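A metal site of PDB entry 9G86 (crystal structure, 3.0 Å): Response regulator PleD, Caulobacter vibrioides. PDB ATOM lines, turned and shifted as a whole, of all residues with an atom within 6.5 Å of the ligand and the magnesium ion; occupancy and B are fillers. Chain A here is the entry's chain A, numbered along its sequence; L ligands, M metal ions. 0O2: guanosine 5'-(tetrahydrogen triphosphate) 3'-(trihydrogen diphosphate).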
ATOM      1  N   LEU A 293     -18.790  29.202   6.373  1.00  0.00           N
ATOM      2  CA  LEU A 293     -19.800  28.271   5.890  1.00  0.00           C
ATOM      3  C   LEU A 293     -21.201  28.780   6.208  1.00  0.00           C
ATOM      4  O   LEU A 293     -21.984  29.112   5.305  1.00  0.00           O
ATOM      5  CB  LEU A 293     -19.553  26.882   6.487  1.00  0.00           C
ATOM      6  CG  LEU A 293     -20.569  25.804   6.136  1.00  0.00           C
ATOM      7  CD1 LEU A 293     -20.338  25.328   4.716  1.00  0.00           C
ATOM      8  CD2 LEU A 293     -20.455  24.641   7.101  1.00  0.00           C
ATOM      9  N   ASP A 326     -27.585  21.464  19.673  1.00  0.00           N
ATOM     10  CA  ASP A 326     -26.764  20.433  19.046  1.00  0.00           C
ATOM     11  C   ASP A 326     -27.611  19.566  18.135  1.00  0.00           C
ATOM     12  O   ASP A 326     -28.608  18.987  18.580  1.00  0.00           O
ATOM     13  CB  ASP A 326     -26.066  19.579  20.097  1.00  0.00           C
ATOM     14  CG  ASP A 326     -24.913  18.797  19.534  1.00  0.00           C
ATOM     15  OD1 ASP A 326     -23.879  19.404  19.181  1.00  0.00           O
ATOM     16  OD2 ASP A 326     -25.057  17.563  19.451  1.00  0.00           O
ATOM     17  N   ILE A 327     -27.223  19.490  16.858  1.00  0.00           N
ATOM     18  CA  ILE A 327     -27.909  18.607  15.935  1.00  0.00           C
ATOM     19  C   ILE A 327     -27.705  17.165  16.379  1.00  0.00           C
ATOM     20  O   ILE A 327     -26.633  16.799  16.874  1.00  0.00           O
ATOM     21  CB  ILE A 327     -27.384  18.847  14.508  1.00  0.00           C
ATOM     22  CG1 ILE A 327     -27.559  20.327  14.137  1.00  0.00           C
ATOM     23  CG2 ILE A 327     -28.092  17.976  13.498  1.00  0.00           C
ATOM     24  CD1 ILE A 327     -27.194  20.665  12.718  1.00  0.00           C
ATOM     25  N   ASP A 328     -28.742  16.334  16.207  1.00  0.00           N
ATOM     26  CA  ASP A 328     -28.721  14.945  16.662  1.00  0.00           C
ATOM     27  C   ASP A 328     -28.357  14.036  15.493  1.00  0.00           C
ATOM     28  O   ASP A 328     -28.961  14.137  14.424  1.00  0.00           O
ATOM     29  CB  ASP A 328     -30.079  14.541  17.234  1.00  0.00           C
ATOM     30  CG  ASP A 328     -30.513  15.403  18.415  1.00  0.00           C
ATOM     31  OD1 ASP A 328     -29.627  15.912  19.142  1.00  0.00           O
ATOM     32  OD2 ASP A 328     -31.741  15.553  18.620  1.00  0.00           O
ATOM     33  N   PHE A 329     -27.392  13.149  15.722  1.00  0.00           N
ATOM     34  CA  PHE A 329     -26.951  12.183  14.718  1.00  0.00           C
ATOM     35  C   PHE A 329     -26.437  12.861  13.450  1.00  0.00           C
ATOM     36  O   PHE A 329     -26.857  12.533  12.334  1.00  0.00           O
ATOM     37  CB  PHE A 329     -28.064  11.189  14.370  1.00  0.00           C
ATOM     38  CG  PHE A 329     -28.713  10.551  15.557  1.00  0.00           C
ATOM     39  CD1 PHE A 329     -27.954   9.815  16.458  1.00  0.00           C
ATOM     40  CD2 PHE A 329     -30.085  10.635  15.755  1.00  0.00           C
ATOM     41  CE1 PHE A 329     -28.540   9.204  17.543  1.00  0.00           C
ATOM     42  CE2 PHE A 329     -30.677  10.021  16.846  1.00  0.00           C
ATOM     43  CZ  PHE A 329     -29.904   9.309  17.742  1.00  0.00           C
ATOM     44  N   PHE A 330     -25.518  13.813  13.623  1.00  0.00           N
ATOM     45  CA  PHE A 330     -24.934  14.441  12.443  1.00  0.00           C
ATOM     46  C   PHE A 330     -23.913  13.520  11.794  1.00  0.00           C
ATOM     47  O   PHE A 330     -23.746  13.552  10.557  1.00  0.00           O
ATOM     48  CB  PHE A 330     -24.293  15.782  12.817  1.00  0.00           C
ATOM     49  CG  PHE A 330     -24.090  16.700  11.650  1.00  0.00           C
ATOM     50  CD1 PHE A 330     -25.116  17.545  11.227  1.00  0.00           C
ATOM     51  CD2 PHE A 330     -22.886  16.717  10.975  1.00  0.00           C
ATOM     52  CE1 PHE A 330     -24.929  18.388  10.143  1.00  0.00           C
ATOM     53  CE2 PHE A 330     -22.700  17.560   9.890  1.00  0.00           C
ATOM     54  CZ  PHE A 330     -23.725  18.390   9.475  1.00  0.00           C
ATOM     55  N   LYS A 331     -23.222  12.715  12.599  1.00  0.00           N
ATOM     56  CA  LYS A 331     -22.271  11.747  12.051  1.00  0.00           C
ATOM     57  C   LYS A 331     -22.951  10.827  11.045  1.00  0.00           C
ATOM     58  O   LYS A 331     -22.332  10.441  10.051  1.00  0.00           O
ATOM     59  CB  LYS A 331     -21.616  10.940  13.170  1.00  0.00           C
ATOM     60  CG  LYS A 331     -20.595  11.725  13.976  1.00  0.00           C
ATOM     61  CD  LYS A 331     -19.914  10.836  15.010  1.00  0.00           C
ATOM     62  CE  LYS A 331     -19.163  11.659  16.041  1.00  0.00           C
ATOM     63  NZ  LYS A 331     -19.593  11.354  17.426  1.00  0.00           N
ATOM     64  N   LYS A 332     -24.209  10.445  11.300  1.00  0.00           N
ATOM     65  CA  LYS A 332     -24.926   9.621  10.331  1.00  0.00           C
ATOM     66  C   LYS A 332     -25.151  10.378   9.033  1.00  0.00           C
ATOM     67  O   LYS A 332     -25.050   9.799   7.938  1.00  0.00           O
ATOM     68  CB  LYS A 332     -26.255   9.161  10.920  1.00  0.00           C
ATOM     69  CG  LYS A 332     -26.944   8.065  10.102  1.00  0.00           C
ATOM     70  CD  LYS A 332     -26.070   6.820   9.967  1.00  0.00           C
ATOM     71  CE  LYS A 332     -26.789   5.704   9.212  1.00  0.00           C
ATOM     72  NZ  LYS A 332     -28.152   5.458   9.764  1.00  0.00           N
ATOM     73  N   ASN A 334     -23.157  12.658   7.763  1.00  0.00           N
ATOM     74  CA  ASN A 334     -21.902  12.633   7.030  1.00  0.00           C
ATOM     75  C   ASN A 334     -21.602  11.243   6.470  1.00  0.00           C
ATOM     76  O   ASN A 334     -21.299  11.112   5.290  1.00  0.00           O
ATOM     77  CB  ASN A 334     -20.753  13.092   7.927  1.00  0.00           C
ATOM     78  CG  ASN A 334     -20.689  14.603   8.074  1.00  0.00           C
ATOM     79  OD1 ASN A 334     -21.092  15.343   7.180  1.00  0.00           O
ATOM     80  ND2 ASN A 334     -20.214  15.070   9.219  1.00  0.00           N
ATOM     81  N   ASP A 335     -21.862  10.196   7.262  1.00  0.00           N
ATOM     82  CA  ASP A 335     -21.571   8.837   6.839  1.00  0.00           C
ATOM     83  C   ASP A 335     -22.412   8.452   5.629  1.00  0.00           C
ATOM     84  O   ASP A 335     -21.966   7.657   4.794  1.00  0.00           O
ATOM     85  CB  ASP A 335     -21.834   7.858   7.978  1.00  0.00           C
ATOM     86  CG  ASP A 335     -20.803   7.950   9.076  1.00  0.00           C
ATOM     87  OD1 ASP A 335     -19.732   8.530   8.834  1.00  0.00           O
ATOM     88  OD2 ASP A 335     -21.079   7.440  10.182  1.00  0.00           O
ATOM     89  N   GLY A 338     -22.144  12.341   2.798  1.00  0.00           N
ATOM     90  CA  GLY A 338     -20.908  13.044   2.536  1.00  0.00           C
ATOM     91  C   GLY A 338     -20.808  14.358   3.297  1.00  0.00           C
ATOM     92  O   GLY A 338     -21.808  14.961   3.706  1.00  0.00           O
ATOM     93  N   HIS A 339     -19.576  14.825   3.448  1.00  0.00           N
ATOM     94  CA  HIS A 339     -19.337  16.054   4.202  1.00  0.00           C
ATOM     95  C   HIS A 339     -19.918  17.262   3.496  1.00  0.00           C
ATOM     96  O   HIS A 339     -20.319  18.214   4.153  1.00  0.00           O
ATOM     97  CB  HIS A 339     -17.854  16.241   4.467  1.00  0.00           C
ATOM     98  CG  HIS A 339     -17.352  15.430   5.612  1.00  0.00           C
ATOM     99  ND1 HIS A 339     -17.345  14.051   5.593  1.00  0.00           N
ATOM    100  CD2 HIS A 339     -16.852  15.795   6.821  1.00  0.00           C
ATOM    101  CE1 HIS A 339     -16.863  13.604   6.738  1.00  0.00           C
ATOM    102  NE2 HIS A 339     -16.557  14.635   7.495  1.00  0.00           N
ATOM    103  N   ASP A 340     -19.917  17.257   2.157  1.00  0.00           N
ATOM    104  CA  ASP A 340     -20.458  18.397   1.427  1.00  0.00           C
ATOM    105  C   ASP A 340     -21.949  18.575   1.699  1.00  0.00           C
ATOM    106  O   ASP A 340     -22.428  19.699   1.925  1.00  0.00           O
ATOM    107  CB  ASP A 340     -20.170  18.215  -0.067  1.00  0.00           C
ATOM    108  CG  ASP A 340     -18.684  18.298  -0.385  1.00  0.00           C
ATOM    109  OD1 ASP A 340     -17.898  18.666   0.517  1.00  0.00           O
ATOM    110  OD2 ASP A 340     -18.304  18.000  -1.538  1.00  0.00           O
ATOM    111  N   ILE A 341     -22.695  17.474   1.682  1.00  0.00           N
ATOM    112  CA  ILE A 341     -24.111  17.538   2.032  1.00  0.00           C
ATOM    113  C   ILE A 341     -24.269  17.984   3.479  1.00  0.00           C
ATOM    114  O   ILE A 341     -25.173  18.757   3.809  1.00  0.00           O
ATOM    115  CB  ILE A 341     -24.813  16.204   1.763  1.00  0.00           C
ATOM    116  CG1 ILE A 341     -25.231  16.083   0.291  1.00  0.00           C
ATOM    117  CG2 ILE A 341     -26.052  16.071   2.644  1.00  0.00           C
ATOM    118  CD1 ILE A 341     -24.076  16.135  -0.706  1.00  0.00           C
ATOM    119  N   GLY A 342     -23.400  17.473   4.368  1.00  0.00           N
ATOM    120  CA  GLY A 342     -23.457  17.930   5.757  1.00  0.00           C
ATOM    121  C   GLY A 342     -23.253  19.429   5.887  1.00  0.00           C
ATOM    122  O   GLY A 342     -23.941  20.091   6.663  1.00  0.00           O
ATOM    123  N   ASP A 343     -22.314  19.979   5.112  1.00  0.00           N
ATOM    124  CA  ASP A 343     -22.113  21.421   5.068  1.00  0.00           C
ATOM    125  C   ASP A 343     -23.367  22.142   4.589  1.00  0.00           C
ATOM    126  O   ASP A 343     -23.718  23.202   5.140  1.00  0.00           O
ATOM    127  CB  ASP A 343     -20.931  21.739   4.144  1.00  0.00           C
ATOM    128  CG  ASP A 343     -19.601  21.246   4.696  1.00  0.00           C
ATOM    129  OD1 ASP A 343     -19.621  20.427   5.645  1.00  0.00           O
ATOM    130  OD2 ASP A 343     -18.539  21.642   4.158  1.00  0.00           O
ATOM    131  N   LEU A 346     -25.787  22.242   7.444  1.00  0.00           N
ATOM    132  CA  LEU A 346     -25.399  23.256   8.418  1.00  0.00           C
ATOM    133  C   LEU A 346     -25.761  24.664   7.951  1.00  0.00           C
ATOM    134  O   LEU A 346     -26.291  25.463   8.723  1.00  0.00           O
ATOM    135  CB  LEU A 346     -23.904  23.151   8.721  1.00  0.00           C
ATOM    136  CG  LEU A 346     -23.487  21.962   9.586  1.00  0.00           C
ATOM    137  CD1 LEU A 346     -21.975  21.874   9.680  1.00  0.00           C
ATOM    138  CD2 LEU A 346     -24.144  22.032  10.953  1.00  0.00           C
ATOM    139  N   ARG A 365     -22.224  30.231  15.689  1.00  0.00           N
ATOM    140  CA  ARG A 365     -21.769  28.837  15.595  1.00  0.00           C
ATOM    141  C   ARG A 365     -20.820  28.563  16.756  1.00  0.00           C
ATOM    142  O   ARG A 365     -19.662  28.991  16.731  1.00  0.00           O
ATOM    143  CB  ARG A 365     -21.114  28.588  14.246  1.00  0.00           C
ATOM    144  CG  ARG A 365     -21.072  27.123  13.843  1.00  0.00           C
ATOM    145  CD  ARG A 365     -20.093  26.893  12.696  1.00  0.00           C
ATOM    146  NE  ARG A 365     -19.832  25.472  12.507  1.00  0.00           N
ATOM    147  CZ  ARG A 365     -19.259  24.939  11.432  1.00  0.00           C
ATOM    148  NH1 ARG A 365     -18.884  25.690  10.412  1.00  0.00           N
ATOM    149  NH2 ARG A 365     -19.076  23.623  11.376  1.00  0.00           N
ATOM    150  N   GLY A 367     -19.769  25.461  17.914  1.00  0.00           N
ATOM    151  CA  GLY A 367     -18.841  24.381  17.629  1.00  0.00           C
ATOM    152  C   GLY A 367     -18.959  23.927  16.191  1.00  0.00           C
ATOM    153  O   GLY A 367     -19.308  24.731  15.320  1.00  0.00           O
ATOM    154  N   GLY A 368     -18.693  22.656  15.929  1.00  0.00           N
ATOM    155  CA  GLY A 368     -18.776  22.196  14.565  1.00  0.00           C
ATOM    156  C   GLY A 368     -20.206  21.959  14.127  1.00  0.00           C
ATOM    157  O   GLY A 368     -20.636  22.444  13.077  1.00  0.00           O
ATOM    158  N   GLU A 369     -20.967  21.236  14.950  1.00  0.00           N
ATOM    159  CA  GLU A 369     -22.378  20.979  14.723  1.00  0.00           C
ATOM    160  C   GLU A 369     -23.249  21.681  15.750  1.00  0.00           C
ATOM    161  O   GLU A 369     -24.475  21.483  15.756  1.00  0.00           O
ATOM    162  CB  GLU A 369     -22.675  19.489  14.741  1.00  0.00           C
ATOM    163  CG  GLU A 369     -22.539  18.867  16.117  1.00  0.00           C
ATOM    164  CD  GLU A 369     -23.540  17.757  16.348  1.00  0.00           C
ATOM    165  OE1 GLU A 369     -24.319  17.462  15.412  1.00  0.00           O
ATOM    166  OE2 GLU A 369     -23.515  17.153  17.421  1.00  0.00           O
ATOM    167  N   SER A 413     -31.199  18.817  19.913  1.00  0.00           N
ATOM    168  CA  SER A 413     -31.331  18.863  21.364  1.00  0.00           C
ATOM    169  C   SER A 413     -30.857  20.226  21.850  1.00  0.00           C
ATOM    170  O   SER A 413     -29.781  20.682  21.455  1.00  0.00           O
ATOM    171  CB  SER A 413     -30.532  17.750  22.032  1.00  0.00           C
ATOM    172  OG  SER A 413     -30.918  16.478  21.554  1.00  0.00           O
ATOM    173  N   LYS A 441     -29.687  14.992  25.491  1.00  0.00           N
ATOM    174  CA  LYS A 441     -29.175  13.887  24.680  1.00  0.00           C
ATOM    175  C   LYS A 441     -29.394  12.546  25.378  1.00  0.00           C
ATOM    176  O   LYS A 441     -29.655  11.532  24.714  1.00  0.00           O
ATOM    177  CB  LYS A 441     -27.693  14.106  24.361  1.00  0.00           C
ATOM    178  N   ARG A 445     -33.944  12.240  22.453  1.00  0.00           N
ATOM    179  CA  ARG A 445     -33.436  13.436  21.776  1.00  0.00           C
ATOM    180  C   ARG A 445     -34.647  14.296  21.415  1.00  0.00           C
ATOM    181  O   ARG A 445     -35.742  14.082  21.932  1.00  0.00           O
ATOM    182  CB  ARG A 445     -32.527  13.058  20.597  1.00  0.00           C
ATOM    183  CG  ARG A 445     -31.195  12.470  21.050  1.00  0.00           C
ATOM    184  CD  ARG A 445     -30.328  12.014  19.897  1.00  0.00           C
ATOM    185  NE  ARG A 445     -28.959  11.786  20.345  1.00  0.00           N
ATOM    186  CZ  ARG A 445     -28.544  10.708  20.996  1.00  0.00           C
ATOM    187  NH1 ARG A 445     -29.363   9.692  21.239  1.00  0.00           N
ATOM    188  NH2 ARG A 445     -27.281  10.636  21.398  1.00  0.00           N
HETATM  189  PD  0O2 L   1     -17.127  13.482  10.663  1.00  0.00           P
HETATM  190  O1D 0O2 L   1     -18.051  14.665  10.490  1.00  0.00           O
HETATM  191  O2D 0O2 L   1     -17.942  12.235  10.936  1.00  0.00           O
HETATM  192  O3D 0O2 L   1     -16.237  13.296   9.465  1.00  0.00           O
HETATM  193  PG  0O2 L   1     -25.362  13.360  18.847  1.00  0.00           P
HETATM  194  O1G 0O2 L   1     -24.132  12.943  19.614  1.00  0.00           O
HETATM  195  O2G 0O2 L   1     -26.396  12.259  18.933  1.00  0.00           O
HETATM  196  O3G 0O2 L   1     -25.904  14.641  19.432  1.00  0.00           O
HETATM  197  PB  0O2 L   1     -23.468  13.616  16.683  1.00  0.00           P
HETATM  198  O1B 0O2 L   1     -23.454  14.233  15.318  1.00  0.00           O
HETATM  199  O2B 0O2 L   1     -22.926  12.206  16.607  1.00  0.00           O
HETATM  200  O3B 0O2 L   1     -25.001  13.600  17.248  1.00  0.00           O
HETATM  201  O3A 0O2 L   1     -22.561  14.474  17.777  1.00  0.00           O
HETATM  202  PA  0O2 L   1     -21.139  15.249  17.506  1.00  0.00           P
HETATM  203  O1A 0O2 L   1     -19.982  14.289  17.610  1.00  0.00           O
HETATM  204  O2A 0O2 L   1     -21.012  16.318  18.561  1.00  0.00           O
HETATM  205  O5' 0O2 L   1     -21.150  15.939  16.004  1.00  0.00           O
HETATM  206  C5' 0O2 L   1     -19.976  16.528  15.471  1.00  0.00           C
HETATM  207  C4' 0O2 L   1     -19.848  16.108  14.152  1.00  0.00           C
HETATM  208  O4' 0O2 L   1     -20.203  17.183  13.151  1.00  0.00           O
HETATM  209  C3' 0O2 L   1     -18.321  15.760  13.853  1.00  0.00           C
HETATM  210  O3' 0O2 L   1     -18.262  14.373  13.298  1.00  0.00           O
HETATM  211  C2' 0O2 L   1     -17.918  16.626  13.044  1.00  0.00           C
HETATM  212  O2' 0O2 L   1     -16.964  16.187  11.997  1.00  0.00           O
HETATM  213  C1' 0O2 L   1     -19.245  17.206  12.258  1.00  0.00           C
HETATM  214  N9  0O2 L   1     -18.880  18.537  11.927  1.00  0.00           N
HETATM  215  C8  0O2 L   1     -18.413  19.616  12.569  1.00  0.00           C
HETATM  216  N7  0O2 L   1     -18.237  20.598  11.654  1.00  0.00           N
HETATM  217  C5  0O2 L   1     -18.596  20.111  10.466  1.00  0.00           C
HETATM  218  C6  0O2 L   1     -18.625  20.751   9.083  1.00  0.00           C
HETATM  219  O6  0O2 L   1     -18.285  21.880   8.929  1.00  0.00           O
HETATM  220  N1  0O2 L   1     -19.056  19.986   7.963  1.00  0.00           N
HETATM  221  C2  0O2 L   1     -19.470  18.616   8.157  1.00  0.00           C
HETATM  222  N2  0O2 L   1     -19.916  17.818   7.036  1.00  0.00           N
HETATM  223  N3  0O2 L   1     -19.445  18.009   9.477  1.00  0.00           N
HETATM  224  C4  0O2 L   1     -18.988  18.817  10.642  1.00  0.00           C
HETATM  225  PC  0O2 L   1     -16.799  13.667  13.416  1.00  0.00           P
HETATM  226  O1C 0O2 L   1     -15.975  14.454  14.398  1.00  0.00           O
HETATM  227  O2C 0O2 L   1     -16.958  12.203  13.780  1.00  0.00           O
HETATM  228  O3C 0O2 L   1     -16.141  13.774  11.925  1.00  0.00           O
HETATM  229 MG    MG M   1     -24.878  15.882  17.771  1.00  0.00          MG
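An oxygen (O6) of the ligand is in hydrogen-bond range of the guanidinium group (NH2) of Arg 365, 3.1 Å away. The side-chain amino group of Lys 331 is in salt-bridge range of an oxygen (O1A) of the ligand (3.0 Å). OD1 of Asp 343 sits at hydrogen-bond distance from N1 of the ligand, at 2.4 Å. The guanidinium group (NE) of Arg 445 is in salt-bridge range of an oxygen (O2G) of the ligand. NE2 of His 339 is in hydrogen-bond range of O3D of the ligand (2.4 Å). O1D of the ligand is in hydrogen-bond range of ND2 of Asn 334 (2.5 Å). An oxygen (O1B) of the ligand sits at hydrogen-bond distance from the backbone NH of Lys 331 (3.1 Å). N of Phe 330 sits at hydrogen-bond distance from O1B of the ligand (2.7 Å). O2G of the ligand lies within hydrogen-bond range of N of Phe 329, at 3.5 Å. A nitrogen (N2) of the ligand lies within hydrogen-bond range of the backbone carbonyl oxygen (O) of His 339 (2.9 Å).
OE2 of Glu 369 binds the magnesium ion, at 1.9 Å. The magnesium ion is bound by O of Ile 327, at 2.2 Å. O3G of the ligand binds the magnesium ion, at 2.3 Å. The magnesium ion is bound by an oxygen (O3B) of the ligand (2.3 Å). The magnesium ion is bound by the side-chain carboxylate (OD2) of Asp 326 (2.4 Å). Slightly farther from the magnesium ion lies O3A of the ligand (2.7 Å).
The backbone carbonyl oxygen of Asp 326 sits at hydrogen-bond distance from the backbone NH of Ser 413. NH2 of Arg 365 lies within hydrogen-bond range of O of Gly 368 (2.6 Å). OG of Ser 413 lies within hydrogen-bond range of OD1 of Asp 328. The guanidinium group (NE) of Arg 365 sits at hydrogen-bond distance from the backbone carbonyl oxygen (O) of Gly 367, at 3.0 Å.
N7 of the ligand lies close to O of Gly 368 (3.3 Å). Merely in contact with the ligand: Leu 346 (3.6 Å), Gly 342 (3.8 Å), Asp 328 (3.8 Å) and Leu 293 (3.96 Å). Hydrophobic or aromatic side chains that line the ligand: Leu 293, Phe 329, Phe 330, His 339 and Leu 346. 16 residues have an atom within 4 Å of the ligand: Leu 293, Asp 326, Ile 327, Asp 328, Phe 329, Phe 330, Lys 331, Asn 334, His 339, Gly 342, Asp 343, Leu 346, Arg 365, Gly 368, Glu 369 and Arg 445. The nearest printed residue that does not touch the ligand is Asp 335 (4.6 Å).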
